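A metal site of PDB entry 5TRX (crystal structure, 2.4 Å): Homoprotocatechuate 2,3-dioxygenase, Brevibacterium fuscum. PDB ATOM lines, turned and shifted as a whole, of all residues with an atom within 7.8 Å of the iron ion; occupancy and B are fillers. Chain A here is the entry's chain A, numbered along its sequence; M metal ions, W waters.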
ATOM      1  N   ASP A 154     -23.276 -12.755   0.774  1.00  0.00           N
ATOM      2  CA  ASP A 154     -24.510 -13.415   1.274  1.00  0.00           C
ATOM      3  C   ASP A 154     -25.044 -12.835   2.578  1.00  0.00           C
ATOM      4  O   ASP A 154     -26.264 -12.653   2.708  1.00  0.00           O
ATOM      5  CB  ASP A 154     -24.348 -14.939   1.413  1.00  0.00           C
ATOM      6  CG  ASP A 154     -25.659 -15.637   1.723  1.00  0.00           C
ATOM      7  OD1 ASP A 154     -26.451 -15.835   0.800  1.00  0.00           O
ATOM      8  OD2 ASP A 154     -25.904 -15.950   2.912  1.00  0.00           O
ATOM      9  N   HIS A 155     -24.184 -12.565   3.569  1.00  0.00           N
ATOM     10  CA  HIS A 155     -24.712 -12.246   4.879  1.00  0.00           C
ATOM     11  C   HIS A 155     -23.681 -11.766   5.901  1.00  0.00           C
ATOM     12  O   HIS A 155     -22.492 -12.024   5.746  1.00  0.00           O
ATOM     13  CB  HIS A 155     -25.509 -13.457   5.422  1.00  0.00           C
ATOM     14  CG  HIS A 155     -24.662 -14.630   5.866  1.00  0.00           C
ATOM     15  ND1 HIS A 155     -24.470 -15.756   5.090  1.00  0.00           N
ATOM     16  CD2 HIS A 155     -24.011 -14.873   7.037  1.00  0.00           C
ATOM     17  CE1 HIS A 155     -23.740 -16.636   5.760  1.00  0.00           C
ATOM     18  NE2 HIS A 155     -23.458 -16.122   6.950  1.00  0.00           N
ATOM     19  N   PHE A 156     -24.155 -11.094   6.948  1.00  0.00           N
ATOM     20  CA  PHE A 156     -23.352 -10.786   8.154  1.00  0.00           C
ATOM     21  C   PHE A 156     -23.728 -11.672   9.318  1.00  0.00           C
ATOM     22  O   PHE A 156     -24.826 -12.246   9.345  1.00  0.00           O
ATOM     23  CB  PHE A 156     -23.577  -9.335   8.597  1.00  0.00           C
ATOM     24  CG  PHE A 156     -23.423  -8.332   7.499  1.00  0.00           C
ATOM     25  CD1 PHE A 156     -22.267  -8.298   6.721  1.00  0.00           C
ATOM     26  CD2 PHE A 156     -24.432  -7.418   7.232  1.00  0.00           C
ATOM     27  CE1 PHE A 156     -22.129  -7.358   5.709  1.00  0.00           C
ATOM     28  CE2 PHE A 156     -24.300  -6.468   6.227  1.00  0.00           C
ATOM     29  CZ  PHE A 156     -23.154  -6.447   5.460  1.00  0.00           C
ATOM     30  N   ASN A 157     -22.842 -11.770  10.298  1.00  0.00           N
ATOM     31  CA  ASN A 157     -23.201 -12.359  11.599  1.00  0.00           C
ATOM     32  C   ASN A 157     -22.634 -11.528  12.726  1.00  0.00           C
ATOM     33  O   ASN A 157     -21.443 -11.219  12.723  1.00  0.00           O
ATOM     34  CB  ASN A 157     -22.695 -13.794  11.694  1.00  0.00           C
ATOM     35  CG  ASN A 157     -23.302 -14.576  12.848  1.00  0.00           C
ATOM     36  OD1 ASN A 157     -23.250 -14.173  14.016  1.00  0.00           O
ATOM     37  ND2 ASN A 157     -23.904 -15.731  12.509  1.00  0.00           N
ATOM     38  N   TRP A 192     -31.477 -16.507  12.928  1.00  0.00           N
ATOM     39  CA  TRP A 192     -31.105 -16.267  11.543  1.00  0.00           C
ATOM     40  C   TRP A 192     -32.281 -15.575  10.876  1.00  0.00           C
ATOM     41  O   TRP A 192     -33.432 -16.050  11.036  1.00  0.00           O
ATOM     42  CB  TRP A 192     -30.851 -17.600  10.845  1.00  0.00           C
ATOM     43  CG  TRP A 192     -29.490 -18.202  11.048  1.00  0.00           C
ATOM     44  CD1 TRP A 192     -28.422 -18.097  10.207  1.00  0.00           C
ATOM     45  CD2 TRP A 192     -29.062 -18.983  12.157  1.00  0.00           C
ATOM     46  NE1 TRP A 192     -27.348 -18.780  10.733  1.00  0.00           N
ATOM     47  CE2 TRP A 192     -27.713 -19.324  11.941  1.00  0.00           C
ATOM     48  CE3 TRP A 192     -29.681 -19.431  13.330  1.00  0.00           C
ATOM     49  CZ2 TRP A 192     -26.970 -20.109  12.829  1.00  0.00           C
ATOM     50  CZ3 TRP A 192     -28.945 -20.205  14.225  1.00  0.00           C
ATOM     51  CH2 TRP A 192     -27.601 -20.545  13.972  1.00  0.00           C
ATOM     52  N   HIS A 200     -30.526 -16.024   5.176  1.00  0.00           N
ATOM     53  CA  HIS A 200     -30.277 -14.741   5.860  1.00  0.00           C
ATOM     54  C   HIS A 200     -29.459 -13.672   5.160  1.00  0.00           C
ATOM     55  O   HIS A 200     -28.710 -13.925   4.207  1.00  0.00           O
ATOM     56  CB  HIS A 200     -29.718 -14.917   7.284  1.00  0.00           C
ATOM     57  CG  HIS A 200     -28.404 -15.628   7.363  1.00  0.00           C
ATOM     58  ND1 HIS A 200     -27.986 -16.571   6.447  1.00  0.00           N
ATOM     59  CD2 HIS A 200     -27.424 -15.565   8.292  1.00  0.00           C
ATOM     60  CE1 HIS A 200     -26.813 -17.053   6.816  1.00  0.00           C
ATOM     61  NE2 HIS A 200     -26.460 -16.459   7.931  1.00  0.00           N
ATOM     62  N   ALA A 203     -27.603 -12.165  11.210  1.00  0.00           N
ATOM     63  CA  ALA A 203     -27.887 -13.184  12.167  1.00  0.00           C
ATOM     64  C   ALA A 203     -27.248 -12.808  13.482  1.00  0.00           C
ATOM     65  O   ALA A 203     -26.344 -11.986  13.534  1.00  0.00           O
ATOM     66  CB  ALA A 203     -27.375 -14.527  11.670  1.00  0.00           C
ATOM     67  N   THR A 205     -25.617 -14.260  17.140  1.00  0.00           N
ATOM     68  CA  THR A 205     -24.944 -15.321  17.853  1.00  0.00           C
ATOM     69  C   THR A 205     -24.715 -14.829  19.299  1.00  0.00           C
ATOM     70  O   THR A 205     -24.028 -13.819  19.515  1.00  0.00           O
ATOM     71  CB  THR A 205     -23.587 -15.606  17.195  1.00  0.00           C
ATOM     72  OG1 THR A 205     -23.786 -16.065  15.844  1.00  0.00           O
ATOM     73  CG2 THR A 205     -22.797 -16.627  17.998  1.00  0.00           C
ATOM     74  N   HIS A 213     -19.028 -11.204  14.033  1.00  0.00           N
ATOM     75  CA  HIS A 213     -18.536 -12.567  14.043  1.00  0.00           C
ATOM     76  C   HIS A 213     -17.937 -12.918  12.686  1.00  0.00           C
ATOM     77  O   HIS A 213     -16.804 -13.378  12.638  1.00  0.00           O
ATOM     78  CB  HIS A 213     -19.646 -13.577  14.430  1.00  0.00           C
ATOM     79  CG  HIS A 213     -19.092 -14.932  14.756  1.00  0.00           C
ATOM     80  ND1 HIS A 213     -18.780 -15.852  13.777  1.00  0.00           N
ATOM     81  CD2 HIS A 213     -18.715 -15.488  15.934  1.00  0.00           C
ATOM     82  CE1 HIS A 213     -18.256 -16.924  14.338  1.00  0.00           C
ATOM     83  NE2 HIS A 213     -18.210 -16.731  15.643  1.00  0.00           N
ATOM     84  N   HIS A 214     -18.668 -12.709  11.599  1.00  0.00           N
ATOM     85  CA  HIS A 214     -18.072 -12.807  10.265  1.00  0.00           C
ATOM     86  C   HIS A 214     -18.872 -12.110   9.166  1.00  0.00           C
ATOM     87  O   HIS A 214     -20.051 -11.811   9.340  1.00  0.00           O
ATOM     88  CB  HIS A 214     -17.923 -14.255   9.865  1.00  0.00           C
ATOM     89  CG  HIS A 214     -19.213 -15.019   9.864  1.00  0.00           C
ATOM     90  ND1 HIS A 214     -19.634 -15.787  10.933  1.00  0.00           N
ATOM     91  CD2 HIS A 214     -20.176 -15.132   8.929  1.00  0.00           C
ATOM     92  CE1 HIS A 214     -20.786 -16.358  10.647  1.00  0.00           C
ATOM     93  NE2 HIS A 214     -21.149 -15.962   9.440  1.00  0.00           N
ATOM     94  N   VAL A 215     -18.214 -11.899   8.036  1.00  0.00           N
ATOM     95  CA  VAL A 215     -18.877 -11.628   6.749  1.00  0.00           C
ATOM     96  C   VAL A 215     -18.854 -12.880   5.882  1.00  0.00           C
ATOM     97  O   VAL A 215     -17.910 -13.657   5.958  1.00  0.00           O
ATOM     98  CB  VAL A 215     -18.130 -10.516   5.988  1.00  0.00           C
ATOM     99  CG1 VAL A 215     -18.918 -10.107   4.751  1.00  0.00           C
ATOM    100  CG2 VAL A 215     -17.882  -9.330   6.903  1.00  0.00           C
ATOM    101  N   ALA A 216     -19.866 -13.088   5.039  1.00  0.00           N
ATOM    102  CA  ALA A 216     -19.928 -14.322   4.258  1.00  0.00           C
ATOM    103  C   ALA A 216     -20.064 -14.063   2.798  1.00  0.00           C
ATOM    104  O   ALA A 216     -20.866 -13.208   2.415  1.00  0.00           O
ATOM    105  CB  ALA A 216     -21.052 -15.215   4.729  1.00  0.00           C
ATOM    106  N   HIS A 248     -23.689 -27.348   6.981  1.00  0.00           N
ATOM    107  CA  HIS A 248     -24.468 -26.880   8.129  1.00  0.00           C
ATOM    108  C   HIS A 248     -25.735 -27.705   8.353  1.00  0.00           C
ATOM    109  O   HIS A 248     -26.427 -28.078   7.389  1.00  0.00           O
ATOM    110  CB  HIS A 248     -24.894 -25.394   7.952  1.00  0.00           C
ATOM    111  CG  HIS A 248     -23.816 -24.388   8.215  1.00  0.00           C
ATOM    112  ND1 HIS A 248     -23.040 -24.393   9.360  1.00  0.00           N
ATOM    113  CD2 HIS A 248     -23.398 -23.322   7.489  1.00  0.00           C
ATOM    114  CE1 HIS A 248     -22.180 -23.379   9.314  1.00  0.00           C
ATOM    115  NE2 HIS A 248     -22.370 -22.717   8.186  1.00  0.00           N
ATOM    116  N   VAL A 250     -28.345 -25.886  10.467  1.00  0.00           N
ATOM    117  CA  VAL A 250     -28.949 -24.584  10.179  1.00  0.00           C
ATOM    118  C   VAL A 250     -28.478 -23.955   8.844  1.00  0.00           C
ATOM    119  O   VAL A 250     -27.290 -23.719   8.655  1.00  0.00           O
ATOM    120  CB  VAL A 250     -28.643 -23.596  11.316  1.00  0.00           C
ATOM    121  CG1 VAL A 250     -29.077 -22.171  10.946  1.00  0.00           C
ATOM    122  CG2 VAL A 250     -29.368 -24.039  12.578  1.00  0.00           C
ATOM    123  N   SER A 251     -29.443 -23.693   7.946  1.00  0.00           N
ATOM    124  CA  SER A 251     -29.218 -23.165   6.586  1.00  0.00           C
ATOM    125  C   SER A 251     -28.977 -24.232   5.491  1.00  0.00           C
ATOM    126  O   SER A 251     -29.187 -23.933   4.286  1.00  0.00           O
ATOM    127  CB  SER A 251     -28.146 -22.070   6.551  1.00  0.00           C
ATOM    128  OG  SER A 251     -26.835 -22.608   6.496  1.00  0.00           O
ATOM    129  N   TYR A 255     -19.957 -25.078   3.764  1.00  0.00           N
ATOM    130  CA  TYR A 255     -19.323 -23.937   4.455  1.00  0.00           C
ATOM    131  C   TYR A 255     -17.860 -24.158   4.738  1.00  0.00           C
ATOM    132  O   TYR A 255     -17.352 -25.288   4.643  1.00  0.00           O
ATOM    133  CB  TYR A 255     -20.009 -23.603   5.772  1.00  0.00           C
ATOM    134  CG  TYR A 255     -19.674 -24.549   6.911  1.00  0.00           C
ATOM    135  CD1 TYR A 255     -18.598 -24.312   7.753  1.00  0.00           C
ATOM    136  CD2 TYR A 255     -20.462 -25.660   7.180  1.00  0.00           C
ATOM    137  CE1 TYR A 255     -18.307 -25.154   8.818  1.00  0.00           C
ATOM    138  CE2 TYR A 255     -20.171 -26.530   8.214  1.00  0.00           C
ATOM    139  CZ  TYR A 255     -19.081 -26.273   9.039  1.00  0.00           C
ATOM    140  OH  TYR A 255     -18.797 -27.128  10.101  1.00  0.00           O
ATOM    141  N   LEU A 256     -17.234 -23.037   5.094  1.00  0.00           N
ATOM    142  CA  LEU A 256     -15.832 -22.953   5.442  1.00  0.00           C
ATOM    143  C   LEU A 256     -15.602 -21.603   6.133  1.00  0.00           C
ATOM    144  O   LEU A 256     -16.122 -20.588   5.699  1.00  0.00           O
ATOM    145  CB  LEU A 256     -14.984 -23.026   4.172  1.00  0.00           C
ATOM    146  CG  LEU A 256     -13.504 -22.745   4.410  1.00  0.00           C
ATOM    147  CD1 LEU A 256     -12.864 -23.951   5.071  1.00  0.00           C
ATOM    148  CD2 LEU A 256     -12.801 -22.384   3.125  1.00  0.00           C
ATOM    149  N   TYR A 257     -14.802 -21.607   7.195  1.00  0.00           N
ATOM    150  CA  TYR A 257     -14.415 -20.371   7.874  1.00  0.00           C
ATOM    151  C   TYR A 257     -12.895 -20.199   7.802  1.00  0.00           C
ATOM    152  O   TYR A 257     -12.131 -21.108   8.145  1.00  0.00           O
ATOM    153  CB  TYR A 257     -14.883 -20.424   9.317  1.00  0.00           C
ATOM    154  CG  TYR A 257     -16.387 -20.471   9.471  1.00  0.00           C
ATOM    155  CD1 TYR A 257     -17.143 -19.292   9.449  1.00  0.00           C
ATOM    156  CD2 TYR A 257     -17.061 -21.689   9.648  1.00  0.00           C
ATOM    157  CE1 TYR A 257     -18.540 -19.335   9.610  1.00  0.00           C
ATOM    158  CE2 TYR A 257     -18.448 -21.755   9.810  1.00  0.00           C
ATOM    159  CZ  TYR A 257     -19.186 -20.568   9.777  1.00  0.00           C
ATOM    160  OH  TYR A 257     -20.570 -20.610   9.934  1.00  0.00           O
ATOM    161  N   GLU A 267     -16.574 -16.258   5.945  1.00  0.00           N
ATOM    162  CA  GLU A 267     -17.231 -17.522   5.610  1.00  0.00           C
ATOM    163  C   GLU A 267     -17.470 -17.671   4.127  1.00  0.00           C
ATOM    164  O   GLU A 267     -17.853 -16.709   3.442  1.00  0.00           O
ATOM    165  CB  GLU A 267     -18.583 -17.657   6.337  1.00  0.00           C
ATOM    166  CG  GLU A 267     -19.272 -19.021   6.120  1.00  0.00           C
ATOM    167  CD  GLU A 267     -20.564 -19.165   6.886  1.00  0.00           C
ATOM    168  OE1 GLU A 267     -20.987 -18.150   7.503  1.00  0.00           O
ATOM    169  OE2 GLU A 267     -21.146 -20.298   6.877  1.00  0.00           O
ATOM    170  N   ILE A 268     -17.285 -18.891   3.632  1.00  0.00           N
ATOM    171  CA  ILE A 268     -17.666 -19.203   2.277  1.00  0.00           C
ATOM    172  C   ILE A 268     -18.781 -20.242   2.272  1.00  0.00           C
ATOM    173  O   ILE A 268     -18.709 -21.225   2.982  1.00  0.00           O
ATOM    174  CB  ILE A 268     -16.515 -19.806   1.473  1.00  0.00           C
ATOM    175  CG1 ILE A 268     -15.144 -19.295   1.942  1.00  0.00           C
ATOM    176  CG2 ILE A 268     -16.738 -19.564  -0.027  1.00  0.00           C
ATOM    177  CD1 ILE A 268     -14.819 -17.902   1.499  1.00  0.00           C
ATOM    178  N   TYR A 269     -19.777 -20.019   1.422  1.00  0.00           N
ATOM    179  CA  TYR A 269     -21.153 -20.453   1.664  1.00  0.00           C
ATOM    180  C   TYR A 269     -21.725 -20.845   0.317  1.00  0.00           C
ATOM    181  O   TYR A 269     -21.471 -20.152  -0.665  1.00  0.00           O
ATOM    182  CB  TYR A 269     -21.904 -19.259   2.207  1.00  0.00           C
ATOM    183  CG  TYR A 269     -23.289 -19.494   2.762  1.00  0.00           C
ATOM    184  CD1 TYR A 269     -23.486 -19.845   4.102  1.00  0.00           C
ATOM    185  CD2 TYR A 269     -24.415 -19.274   1.975  1.00  0.00           C
ATOM    186  CE1 TYR A 269     -24.766 -19.993   4.618  1.00  0.00           C
ATOM    187  CE2 TYR A 269     -25.668 -19.419   2.482  1.00  0.00           C
ATOM    188  CZ  TYR A 269     -25.855 -19.780   3.801  1.00  0.00           C
ATOM    189  OH  TYR A 269     -27.130 -19.927   4.290  1.00  0.00           O
ATOM    190  N   ARG A 293     -24.980 -27.503  13.792  1.00  0.00           N
ATOM    191  CA  ARG A 293     -24.034 -26.594  13.158  1.00  0.00           C
ATOM    192  C   ARG A 293     -23.169 -27.254  12.072  1.00  0.00           C
ATOM    193  O   ARG A 293     -22.986 -26.662  11.004  1.00  0.00           O
ATOM    194  CB  ARG A 293     -23.132 -25.951  14.202  1.00  0.00           C
ATOM    195  CG  ARG A 293     -23.845 -24.869  14.975  1.00  0.00           C
ATOM    196  CD  ARG A 293     -22.877 -23.981  15.715  1.00  0.00           C
ATOM    197  NE  ARG A 293     -23.608 -23.048  16.548  1.00  0.00           N
ATOM    198  CZ  ARG A 293     -24.140 -21.887  16.164  1.00  0.00           C
ATOM    199  NH1 ARG A 293     -24.056 -21.445  14.917  1.00  0.00           N
ATOM    200  NH2 ARG A 293     -24.777 -21.152  17.061  1.00  0.00           N
ATOM    201  N   TRP A 304     -14.077 -20.451  17.421  1.00  0.00           N
ATOM    202  CA  TRP A 304     -15.333 -20.057  16.785  1.00  0.00           C
ATOM    203  C   TRP A 304     -16.350 -19.457  17.780  1.00  0.00           C
ATOM    204  O   TRP A 304     -17.133 -18.579  17.439  1.00  0.00           O
ATOM    205  CB  TRP A 304     -15.945 -21.226  15.995  1.00  0.00           C
ATOM    206  CG  TRP A 304     -16.902 -20.759  14.938  1.00  0.00           C
ATOM    207  CD1 TRP A 304     -16.604 -20.501  13.648  1.00  0.00           C
ATOM    208  CD2 TRP A 304     -18.302 -20.478  15.097  1.00  0.00           C
ATOM    209  NE1 TRP A 304     -17.744 -20.084  12.964  1.00  0.00           N
ATOM    210  CE2 TRP A 304     -18.793 -20.055  13.831  1.00  0.00           C
ATOM    211  CE3 TRP A 304     -19.197 -20.550  16.168  1.00  0.00           C
ATOM    212  CZ2 TRP A 304     -20.123 -19.670  13.635  1.00  0.00           C
ATOM    213  CZ3 TRP A 304     -20.523 -20.205  15.949  1.00  0.00           C
ATOM    214  CH2 TRP A 304     -20.970 -19.762  14.707  1.00  0.00           C
HETATM  215 FE    FE M   1     -22.642 -17.605   8.661  1.00  0.00          FE
HETATM  216  O   HOH W   1     -23.668 -19.287   7.543  1.00  0.00           O
HETATM  217  O   HOH W   2     -22.973 -19.255  10.500  1.00  0.00           O
HETATM  218  O   HOH W   3     -24.292 -16.918   9.742  1.00  0.00           O
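A ring nitrogen (NE2) of His 200 sits close to a ring nitrogen (NE2) of His 155, 3.2 Å away. ND1 of His 155 is in hydrogen-bond range of OD2 of Asp 154 (2.6 Å). The backbone carbonyl oxygen (O) of His 155 is in hydrogen-bond range of the backbone NH (N) of Ala 216, 2.9 Å away. The side-chain hydroxyl of Tyr 257 lies within hydrogen-bond range of the side-chain carboxylate of Glu 267 (3.1 Å). OH of Tyr 257 lies close to NE2 of His 248. The side-chain carboxylate (OE2) of Glu 267 is in hydrogen-bond range of a ring nitrogen (NE2) of His 248 (3.0 Å). A ring nitrogen (ND1) of His 214 sits at hydrogen-bond distance from a ring nitrogen (ND1) of His 213, 3.0 Å away. N of Glu 267 is in hydrogen-bond range of O of Val 215.
Tyr 257 touches the iron ion (OH to FE, 3.9 Å).
The iron ion is bound by water W3, the side-chain carboxylate (OE1) of Glu 267, water W1, a ring nitrogen (NE2) of His 214, a ring nitrogen (NE2) of His 155 and water W2. The iron ion has six donor atoms within binding distance.
Water W3 bridges NE2 of His 200 and ND2 of Asn 157.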
